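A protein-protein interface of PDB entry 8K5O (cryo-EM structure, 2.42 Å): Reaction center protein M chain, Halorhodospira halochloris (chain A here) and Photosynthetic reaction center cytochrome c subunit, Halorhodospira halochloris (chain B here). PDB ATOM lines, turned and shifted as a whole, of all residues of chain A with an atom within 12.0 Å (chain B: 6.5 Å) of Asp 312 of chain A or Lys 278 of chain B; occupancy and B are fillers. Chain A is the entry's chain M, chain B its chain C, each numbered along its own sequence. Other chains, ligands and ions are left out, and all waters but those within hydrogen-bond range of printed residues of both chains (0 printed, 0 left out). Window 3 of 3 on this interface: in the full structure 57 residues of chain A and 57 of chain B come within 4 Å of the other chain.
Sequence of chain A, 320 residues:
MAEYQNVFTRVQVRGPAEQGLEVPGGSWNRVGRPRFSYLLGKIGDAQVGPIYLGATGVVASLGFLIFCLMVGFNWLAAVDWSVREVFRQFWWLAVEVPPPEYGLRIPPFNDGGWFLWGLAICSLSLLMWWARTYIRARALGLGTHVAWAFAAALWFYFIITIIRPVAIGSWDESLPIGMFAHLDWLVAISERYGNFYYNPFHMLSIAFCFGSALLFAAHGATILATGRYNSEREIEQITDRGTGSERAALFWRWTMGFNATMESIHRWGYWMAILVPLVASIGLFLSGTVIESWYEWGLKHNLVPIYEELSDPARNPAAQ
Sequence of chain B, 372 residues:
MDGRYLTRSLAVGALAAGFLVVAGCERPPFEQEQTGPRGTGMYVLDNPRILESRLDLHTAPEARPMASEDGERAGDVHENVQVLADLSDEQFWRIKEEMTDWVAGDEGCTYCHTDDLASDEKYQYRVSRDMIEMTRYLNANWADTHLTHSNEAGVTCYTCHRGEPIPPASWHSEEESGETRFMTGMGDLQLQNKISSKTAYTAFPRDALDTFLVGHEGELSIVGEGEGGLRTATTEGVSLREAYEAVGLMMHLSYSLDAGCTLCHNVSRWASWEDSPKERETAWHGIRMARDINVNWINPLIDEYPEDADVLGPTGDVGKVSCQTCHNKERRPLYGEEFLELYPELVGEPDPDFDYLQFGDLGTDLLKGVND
The backbone carbonyl oxygen of Ser 276 of chain B lies within hydrogen-bond range of the backbone NH of Ala 314 of chain A (3.1 Å).
NZ of Lys 278 of chain B lies within hydrogen-bond range of O of Pro 313 of chain A (3.4 Å).
The side-chain carboxylate (OE1) of Glu 281 of chain B is in hydrogen-bond range of the backbone NH (N) of Arg 315 of chain A (3.2 Å).
O of Trp 273 of chain B sits close to O of Ala 314 of chain A.
The backbone carbonyl oxygen (O) of Cys 264 of chain B sits close to the side-chain hydroxyl (OG) of Ser 276 of chain B (3.4 Å).
The side-chain sulfur (SG) of Cys 264 of chain B sits at hydrogen-bond distance from the backbone NH (N) of Arg 280 of chain B, at 3.3 Å.
The side-chain hydroxyl of Ser 276 of chain B lies within hydrogen-bond range of the guanidinium group of Arg 280 of chain B (3.0 Å).
The side-chain amide oxygen (OD1) of Asn 316 of chain A sits close to the backbone NH (N) of Ala 318 of chain A (3.2 Å).
CD1 of Leu 310 of chain A touches O of Ser 276 of chain B, 3.4 Å away.
Pro 277 of chain B touches Leu 310 of chain A.
Asp 312 of chain A touches Lys 278 of chain B.
Pro 313 of chain A touches Ser 276 of chain B.
Pro 277 of chain B touches Ala 314 of chain A (O to CB, 3.2 Å).
Ala 314 of chain A touches Lys 278 of chain B.
CB of Ala 314 of chain A touches CB of Arg 280 of chain B, at 3.8 Å.
CB of Ala 314 of chain A touches N of Glu 281 of chain B, at 3.7 Å.
Trp 273 of chain B touches Asn 316 of chain A.
Pro 317 of chain A touches Trp 273 of chain B (CD to CH2, 3.7 Å).
Of the printed residues of chain B, Asp 312 of chain A touches Lys 278 (3.7 Å).
Of chain A, only Asp 312 (3.7 Å), Pro 313 (3.4 Å) and Ala 314 (3.9 Å) come within 4 Å of Lys 278 of chain B.
Ser 276 of chain B touches just these residues of chain A: Leu 310, Pro 313 and Ala 314.
No residue of chain A comes within 4 Å of Glu 279 of chain B.
Thr 282 of chain B touches none of the printed residues of chain A.
Printed residues of chain B within 4 Å of Leu 310 of chain A: Ser 276 and Pro 277.
Of the printed residues of chain B, Pro 317 of chain A touches Trp 273.
The nearest residue of chain B that does not touch Asp 312 of chain A is Pro 277 of chain B (4.9 Å).
The nearest residue of chain A that does not touch Lys 278 of chain B is Arg 315 of chain A (4.03 Å).
Of the 13 printed residues of chain A, 7 touch a printed residue of chain B.
Hydrophobic or aromatic side chains of chain A that line the printed part of chain B: Leu 310, Ala 314 and Pro 317.
Of the 13 printed residues of chain B, 6 touch a printed residue of chain A.
Printed residues of chain B that touch a printed residue of chain A: Trp 273, Ser 276, Pro 277, Lys 278, Arg 280 and Glu 281.
Among the printed residues, 15 pairs touch across the chains.
Among the printed residues, no Asp or Glu carboxylate lies within 4 Å of a Lys or Arg side-chain nitrogen of the other chain.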
ATOM      1  N   TYR A 307       3.157  16.289  12.679  1.00  0.00           N
ATOM      2  CA  TYR A 307       3.383  17.650  13.129  1.00  0.00           C
ATOM      3  C   TYR A 307       4.806  18.089  12.824  1.00  0.00           C
ATOM      4  O   TYR A 307       5.647  17.305  12.384  1.00  0.00           O
ATOM      5  CB  TYR A 307       3.086  17.762  14.623  1.00  0.00           C
ATOM      6  CG  TYR A 307       1.662  17.412  14.944  1.00  0.00           C
ATOM      7  CD1 TYR A 307       0.623  18.211  14.496  1.00  0.00           C
ATOM      8  CD2 TYR A 307       1.352  16.279  15.673  1.00  0.00           C
ATOM      9  CE1 TYR A 307      -0.679  17.900  14.774  1.00  0.00           C
ATOM     10  CE2 TYR A 307       0.048  15.958  15.955  1.00  0.00           C
ATOM     11  CZ  TYR A 307      -0.962  16.774  15.503  1.00  0.00           C
ATOM     12  OH  TYR A 307      -2.267  16.467  15.777  1.00  0.00           O
ATOM     13  N   GLU A 308       5.058  19.373  13.065  1.00  0.00           N
ATOM     14  CA  GLU A 308       6.377  19.940  12.844  1.00  0.00           C
ATOM     15  C   GLU A 308       7.416  19.144  13.615  1.00  0.00           C
ATOM     16  O   GLU A 308       7.225  18.832  14.794  1.00  0.00           O
ATOM     17  CB  GLU A 308       6.392  21.403  13.286  1.00  0.00           C
ATOM     18  CG  GLU A 308       7.358  22.288  12.528  1.00  0.00           C
ATOM     19  CD  GLU A 308       7.110  23.760  12.783  1.00  0.00           C
ATOM     20  OE1 GLU A 308       6.719  24.107  13.918  1.00  0.00           O
ATOM     21  OE2 GLU A 308       7.305  24.572  11.853  1.00  0.00           O
ATOM     22  N   GLU A 309       8.505  18.788  12.938  1.00  0.00           N
ATOM     23  CA  GLU A 309       9.592  18.090  13.606  1.00  0.00           C
ATOM     24  C   GLU A 309      10.139  18.961  14.726  1.00  0.00           C
ATOM     25  O   GLU A 309      10.378  20.158  14.535  1.00  0.00           O
ATOM     26  CB  GLU A 309      10.690  17.731  12.604  1.00  0.00           C
ATOM     27  CG  GLU A 309      11.317  18.917  11.894  1.00  0.00           C
ATOM     28  CD  GLU A 309      12.366  18.510  10.877  1.00  0.00           C
ATOM     29  OE1 GLU A 309      12.607  17.295  10.722  1.00  0.00           O
ATOM     30  OE2 GLU A 309      12.947  19.405  10.230  1.00  0.00           O
ATOM     31  N   LEU A 310      10.303  18.372  15.905  1.00  0.00           N
ATOM     32  CA  LEU A 310      10.774  19.138  17.047  1.00  0.00           C
ATOM     33  C   LEU A 310      12.242  19.496  16.885  1.00  0.00           C
ATOM     34  O   LEU A 310      13.032  18.722  16.340  1.00  0.00           O
ATOM     35  CB  LEU A 310      10.573  18.356  18.343  1.00  0.00           C
ATOM     36  CG  LEU A 310       9.152  17.923  18.689  1.00  0.00           C
ATOM     37  CD1 LEU A 310       9.191  16.827  19.732  1.00  0.00           C
ATOM     38  CD2 LEU A 310       8.333  19.104  19.178  1.00  0.00           C
ATOM     39  N   SER A 311      12.601  20.688  17.346  1.00  0.00           N
ATOM     40  CA  SER A 311      14.006  21.011  17.531  1.00  0.00           C
ATOM     41  C   SER A 311      14.535  20.215  18.714  1.00  0.00           C
ATOM     42  O   SER A 311      13.974  20.275  19.813  1.00  0.00           O
ATOM     43  CB  SER A 311      14.189  22.509  17.766  1.00  0.00           C
ATOM     44  OG  SER A 311      13.668  23.262  16.687  1.00  0.00           O
ATOM     45  N   ASP A 312      15.607  19.460  18.482  1.00  0.00           N
ATOM     46  CA  ASP A 312      16.188  18.577  19.487  1.00  0.00           C
ATOM     47  C   ASP A 312      15.161  17.560  19.978  1.00  0.00           C
ATOM     48  O   ASP A 312      14.706  17.646  21.126  1.00  0.00           O
ATOM     49  CB  ASP A 312      16.740  19.394  20.660  1.00  0.00           C
ATOM     50  CG  ASP A 312      17.901  18.712  21.353  1.00  0.00           C
ATOM     51  OD1 ASP A 312      18.534  17.830  20.737  1.00  0.00           O
ATOM     52  OD2 ASP A 312      18.182  19.062  22.519  1.00  0.00           O
ATOM     53  N   PRO A 313      14.755  16.600  19.148  1.00  0.00           N
ATOM     54  CA  PRO A 313      13.852  15.549  19.623  1.00  0.00           C
ATOM     55  C   PRO A 313      14.548  14.642  20.624  1.00  0.00           C
ATOM     56  O   PRO A 313      15.776  14.556  20.682  1.00  0.00           O
ATOM     57  CB  PRO A 313      13.500  14.773  18.350  1.00  0.00           C
ATOM     58  CG  PRO A 313      13.786  15.698  17.241  1.00  0.00           C
ATOM     59  CD  PRO A 313      14.962  16.512  17.694  1.00  0.00           C
ATOM     60  N   ALA A 314      13.737  13.953  21.420  1.00  0.00           N
ATOM     61  CA  ALA A 314      14.270  12.933  22.310  1.00  0.00           C
ATOM     62  C   ALA A 314      14.666  11.704  21.504  1.00  0.00           C
ATOM     63  O   ALA A 314      13.868  11.176  20.725  1.00  0.00           O
ATOM     64  CB  ALA A 314      13.241  12.558  23.374  1.00  0.00           C
ATOM     65  N   ARG A 315      15.902  11.257  21.679  1.00  0.00           N
ATOM     66  CA  ARG A 315      16.396  10.061  21.013  1.00  0.00           C
ATOM     67  C   ARG A 315      16.341   8.897  21.988  1.00  0.00           C
ATOM     68  O   ARG A 315      16.766   9.026  23.139  1.00  0.00           O
ATOM     69  CB  ARG A 315      17.822  10.267  20.498  1.00  0.00           C
ATOM     70  CG  ARG A 315      17.934  11.332  19.420  1.00  0.00           C
ATOM     71  CD  ARG A 315      19.386  11.693  19.115  1.00  0.00           C
ATOM     72  NE  ARG A 315      20.226  10.545  18.784  1.00  0.00           N
ATOM     73  CZ  ARG A 315      20.020   9.700  17.780  1.00  0.00           C
ATOM     74  NH1 ARG A 315      19.007   9.851  16.940  1.00  0.00           N
ATOM     75  NH2 ARG A 315      20.858   8.682  17.608  1.00  0.00           N
ATOM     76  N   ASN A 316      15.804   7.775  21.533  1.00  0.00           N
ATOM     77  CA  ASN A 316      15.708   6.595  22.379  1.00  0.00           C
ATOM     78  C   ASN A 316      17.108   6.126  22.751  1.00  0.00           C
ATOM     79  O   ASN A 316      17.889   5.774  21.858  1.00  0.00           O
ATOM     80  CB  ASN A 316      14.948   5.490  21.658  1.00  0.00           C
ATOM     81  CG  ASN A 316      14.636   4.310  22.555  1.00  0.00           C
ATOM     82  OD1 ASN A 316      14.908   4.337  23.752  1.00  0.00           O
ATOM     83  ND2 ASN A 316      14.054   3.269  21.978  1.00  0.00           N
ATOM     84  N   PRO A 317      17.470   6.110  24.035  1.00  0.00           N
ATOM     85  CA  PRO A 317      18.808   5.634  24.407  1.00  0.00           C
ATOM     86  C   PRO A 317      19.002   4.151  24.168  1.00  0.00           C
ATOM     87  O   PRO A 317      20.149   3.690  24.150  1.00  0.00           O
ATOM     88  CB  PRO A 317      18.904   5.983  25.897  1.00  0.00           C
ATOM     89  CG  PRO A 317      17.845   7.016  26.115  1.00  0.00           C
ATOM     90  CD  PRO A 317      16.741   6.639  25.196  1.00  0.00           C
ATOM     91  N   ALA A 318      17.921   3.394  23.983  1.00  0.00           N
ATOM     92  CA  ALA A 318      17.994   1.980  23.647  1.00  0.00           C
ATOM     93  C   ALA A 318      17.984   1.739  22.145  1.00  0.00           C
ATOM     94  O   ALA A 318      17.503   0.691  21.692  1.00  0.00           O
ATOM     95  CB  ALA A 318      16.847   1.223  24.316  1.00  0.00           C
ATOM     96  N   ALA A 319      18.493   2.692  21.366  1.00  0.00           N
ATOM     97  CA  ALA A 319      18.521   2.616  19.907  1.00  0.00           C
ATOM     98  C   ALA A 319      17.123   2.413  19.336  1.00  0.00           C
ATOM     99  O   ALA A 319      16.378   3.373  19.147  1.00  0.00           O
ATOM    100  CB  ALA A 319      19.453   1.507  19.443  1.00  0.00           C
ATOM    101  N   THR B  35       5.927  22.399  25.065  1.00  0.00           N
ATOM    102  CA  THR B  35       6.849  21.292  24.855  1.00  0.00           C
ATOM    103  C   THR B  35       6.722  20.661  23.475  1.00  0.00           C
ATOM    104  O   THR B  35       7.542  19.809  23.125  1.00  0.00           O
ATOM    105  CB  THR B  35       6.637  20.220  25.928  1.00  0.00           C
ATOM    106  OG1 THR B  35       5.347  19.624  25.768  1.00  0.00           O
ATOM    107  CG2 THR B  35       6.725  20.832  27.313  1.00  0.00           C
ATOM    108  N   HIS B 149      21.159  17.854  32.763  1.00  0.00           N
ATOM    109  CA  HIS B 149      20.376  18.092  31.556  1.00  0.00           C
ATOM    110  C   HIS B 149      20.286  19.578  31.234  1.00  0.00           C
ATOM    111  O   HIS B 149      20.553  19.996  30.103  1.00  0.00           O
ATOM    112  CB  HIS B 149      18.980  17.492  31.701  1.00  0.00           C
ATOM    113  CG  HIS B 149      18.164  17.572  30.450  1.00  0.00           C
ATOM    114  ND1 HIS B 149      17.040  18.361  30.343  1.00  0.00           N
ATOM    115  CD2 HIS B 149      18.318  16.973  29.246  1.00  0.00           C
ATOM    116  CE1 HIS B 149      16.532  18.238  29.131  1.00  0.00           C
ATOM    117  NE2 HIS B 149      17.289  17.402  28.444  1.00  0.00           N
ATOM    118  N   LEU B 263       5.031  16.810  28.964  1.00  0.00           N
ATOM    119  CA  LEU B 263       6.406  17.220  29.218  1.00  0.00           C
ATOM    120  C   LEU B 263       7.385  16.377  28.419  1.00  0.00           C
ATOM    121  O   LEU B 263       8.359  16.896  27.865  1.00  0.00           O
ATOM    122  CB  LEU B 263       6.715  17.120  30.709  1.00  0.00           C
ATOM    123  CG  LEU B 263       8.180  17.349  31.075  1.00  0.00           C
ATOM    124  CD1 LEU B 263       8.504  18.829  31.001  1.00  0.00           C
ATOM    125  CD2 LEU B 263       8.492  16.792  32.446  1.00  0.00           C
ATOM    126  N   CYS B 264       7.019  15.149  28.186  1.00  0.00           N
ATOM    127  CA  CYS B 264       7.926  14.276  27.541  1.00  0.00           C
ATOM    128  C   CYS B 264       7.307  13.514  26.401  1.00  0.00           C
ATOM    129  O   CYS B 264       7.926  12.616  25.903  1.00  0.00           O
ATOM    130  CB  CYS B 264       8.452  13.388  28.653  1.00  0.00           C
ATOM    131  SG  CYS B 264       9.593  14.369  29.611  1.00  0.00           S
ATOM    132  N   TRP B 273       9.594   8.506  19.689  1.00  0.00           N
ATOM    133  CA  TRP B 273      10.594   9.332  20.353  1.00  0.00           C
ATOM    134  C   TRP B 273      10.866  10.609  19.575  1.00  0.00           C
ATOM    135  O   TRP B 273      11.141  11.652  20.175  1.00  0.00           O
ATOM    136  CB  TRP B 273      11.884   8.541  20.534  1.00  0.00           C
ATOM    137  CG  TRP B 273      11.834   7.572  21.657  1.00  0.00           C
ATOM    138  CD1 TRP B 273      11.261   6.338  21.644  1.00  0.00           C
ATOM    139  CD2 TRP B 273      12.382   7.746  22.966  1.00  0.00           C
ATOM    140  NE1 TRP B 273      11.415   5.731  22.862  1.00  0.00           N
ATOM    141  CE2 TRP B 273      12.101   6.576  23.693  1.00  0.00           C
ATOM    142  CE3 TRP B 273      13.083   8.778  23.594  1.00  0.00           C
ATOM    143  CZ2 TRP B 273      12.498   6.408  25.015  1.00  0.00           C
ATOM    144  CZ3 TRP B 273      13.473   8.610  24.904  1.00  0.00           C
ATOM    145  CH2 TRP B 273      13.179   7.435  25.601  1.00  0.00           C
ATOM    146  N   SER B 276       8.669  13.280  20.715  1.00  0.00           N
ATOM    147  CA  SER B 276       8.720  13.548  22.139  1.00  0.00           C
ATOM    148  C   SER B 276       9.741  14.633  22.454  1.00  0.00           C
ATOM    149  O   SER B 276      10.791  14.713  21.812  1.00  0.00           O
ATOM    150  CB  SER B 276       9.084  12.282  22.916  1.00  0.00           C
ATOM    151  OG  SER B 276       8.113  11.270  22.734  1.00  0.00           O
ATOM    152  N   PRO B 277       9.449  15.483  23.433  1.00  0.00           N
ATOM    153  CA  PRO B 277      10.432  16.477  23.865  1.00  0.00           C
ATOM    154  C   PRO B 277      11.655  15.818  24.484  1.00  0.00           C
ATOM    155  O   PRO B 277      11.600  14.701  24.999  1.00  0.00           O
ATOM    156  CB  PRO B 277       9.668  17.314  24.896  1.00  0.00           C
ATOM    157  CG  PRO B 277       8.234  17.069  24.599  1.00  0.00           C
ATOM    158  CD  PRO B 277       8.141  15.682  24.075  1.00  0.00           C
ATOM    159  N   LYS B 278      12.770  16.552  24.433  1.00  0.00           N
ATOM    160  CA  LYS B 278      14.061  16.021  24.861  1.00  0.00           C
ATOM    161  C   LYS B 278      14.011  15.474  26.281  1.00  0.00           C
ATOM    162  O   LYS B 278      14.749  14.538  26.611  1.00  0.00           O
ATOM    163  CB  LYS B 278      15.121  17.119  24.768  1.00  0.00           C
ATOM    164  CG  LYS B 278      16.555  16.634  24.783  1.00  0.00           C
ATOM    165  CD  LYS B 278      16.782  15.524  23.785  1.00  0.00           C
ATOM    166  CE  LYS B 278      18.257  15.232  23.637  1.00  0.00           C
ATOM    167  NZ  LYS B 278      18.514  14.187  22.610  1.00  0.00           N
ATOM    168  N   GLU B 279      13.139  16.027  27.124  1.00  0.00           N
ATOM    169  CA  GLU B 279      13.052  15.607  28.515  1.00  0.00           C
ATOM    170  C   GLU B 279      12.685  14.139  28.655  1.00  0.00           C
ATOM    171  O   GLU B 279      12.914  13.556  29.716  1.00  0.00           O
ATOM    172  CB  GLU B 279      12.034  16.473  29.254  1.00  0.00           C
ATOM    173  CG  GLU B 279      12.419  17.937  29.332  1.00  0.00           C
ATOM    174  CD  GLU B 279      12.127  18.680  28.045  1.00  0.00           C
ATOM    175  OE1 GLU B 279      10.951  18.714  27.627  1.00  0.00           O
ATOM    176  OE2 GLU B 279      13.076  19.221  27.443  1.00  0.00           O
ATOM    177  N   ARG B 280      12.105  13.535  27.619  1.00  0.00           N
ATOM    178  CA  ARG B 280      11.877  12.097  27.641  1.00  0.00           C
ATOM    179  C   ARG B 280      13.195  11.342  27.727  1.00  0.00           C
ATOM    180  O   ARG B 280      13.370  10.468  28.583  1.00  0.00           O
ATOM    181  CB  ARG B 280      11.094  11.678  26.400  1.00  0.00           C
ATOM    182  CG  ARG B 280      10.372  10.361  26.543  1.00  0.00           C
ATOM    183  CD  ARG B 280      10.045   9.782  25.195  1.00  0.00           C
ATOM    184  NE  ARG B 280       9.661   8.382  25.282  1.00  0.00           N
ATOM    185  CZ  ARG B 280       8.938   7.753  24.369  1.00  0.00           C
ATOM    186  NH1 ARG B 280       8.500   8.373  23.289  1.00  0.00           N
ATOM    187  NH2 ARG B 280       8.643   6.470  24.549  1.00  0.00           N
ATOM    188  N   GLU B 281      14.152  11.698  26.867  1.00  0.00           N
ATOM    189  CA  GLU B 281      15.422  10.982  26.824  1.00  0.00           C
ATOM    190  C   GLU B 281      16.096  10.972  28.189  1.00  0.00           C
ATOM    191  O   GLU B 281      16.426   9.905  28.722  1.00  0.00           O
ATOM    192  CB  GLU B 281      16.334  11.611  25.774  1.00  0.00           C
ATOM    193  CG  GLU B 281      17.801  11.294  25.959  1.00  0.00           C
ATOM    194  CD  GLU B 281      18.558  11.299  24.656  1.00  0.00           C
ATOM    195  OE1 GLU B 281      18.224  12.119  23.778  1.00  0.00           O
ATOM    196  OE2 GLU B 281      19.488  10.480  24.504  1.00  0.00           O
ATOM    197  N   THR B 282      16.265  12.149  28.793  1.00  0.00           N
ATOM    198  CA  THR B 282      16.852  12.206  30.126  1.00  0.00           C
ATOM    199  C   THR B 282      15.991  11.449  31.129  1.00  0.00           C
ATOM    200  O   THR B 282      16.518  10.727  31.986  1.00  0.00           O
ATOM    201  CB  THR B 282      17.073  13.663  30.550  1.00  0.00           C
ATOM    202  OG1 THR B 282      17.591  13.720  31.885  1.00  0.00           O
ATOM    203  CG2 THR B 282      15.808  14.463  30.470  1.00  0.00           C
ATOM    204  N   ALA B 283      14.665  11.557  31.003  1.00  0.00           N
ATOM    205  CA  ALA B 283      13.776  10.784  31.859  1.00  0.00           C
ATOM    206  C   ALA B 283      14.093   9.306  31.759  1.00  0.00           C
ATOM    207  O   ALA B 283      14.143   8.602  32.775  1.00  0.00           O
ATOM    208  CB  ALA B 283      12.322  11.039  31.475  1.00  0.00           C
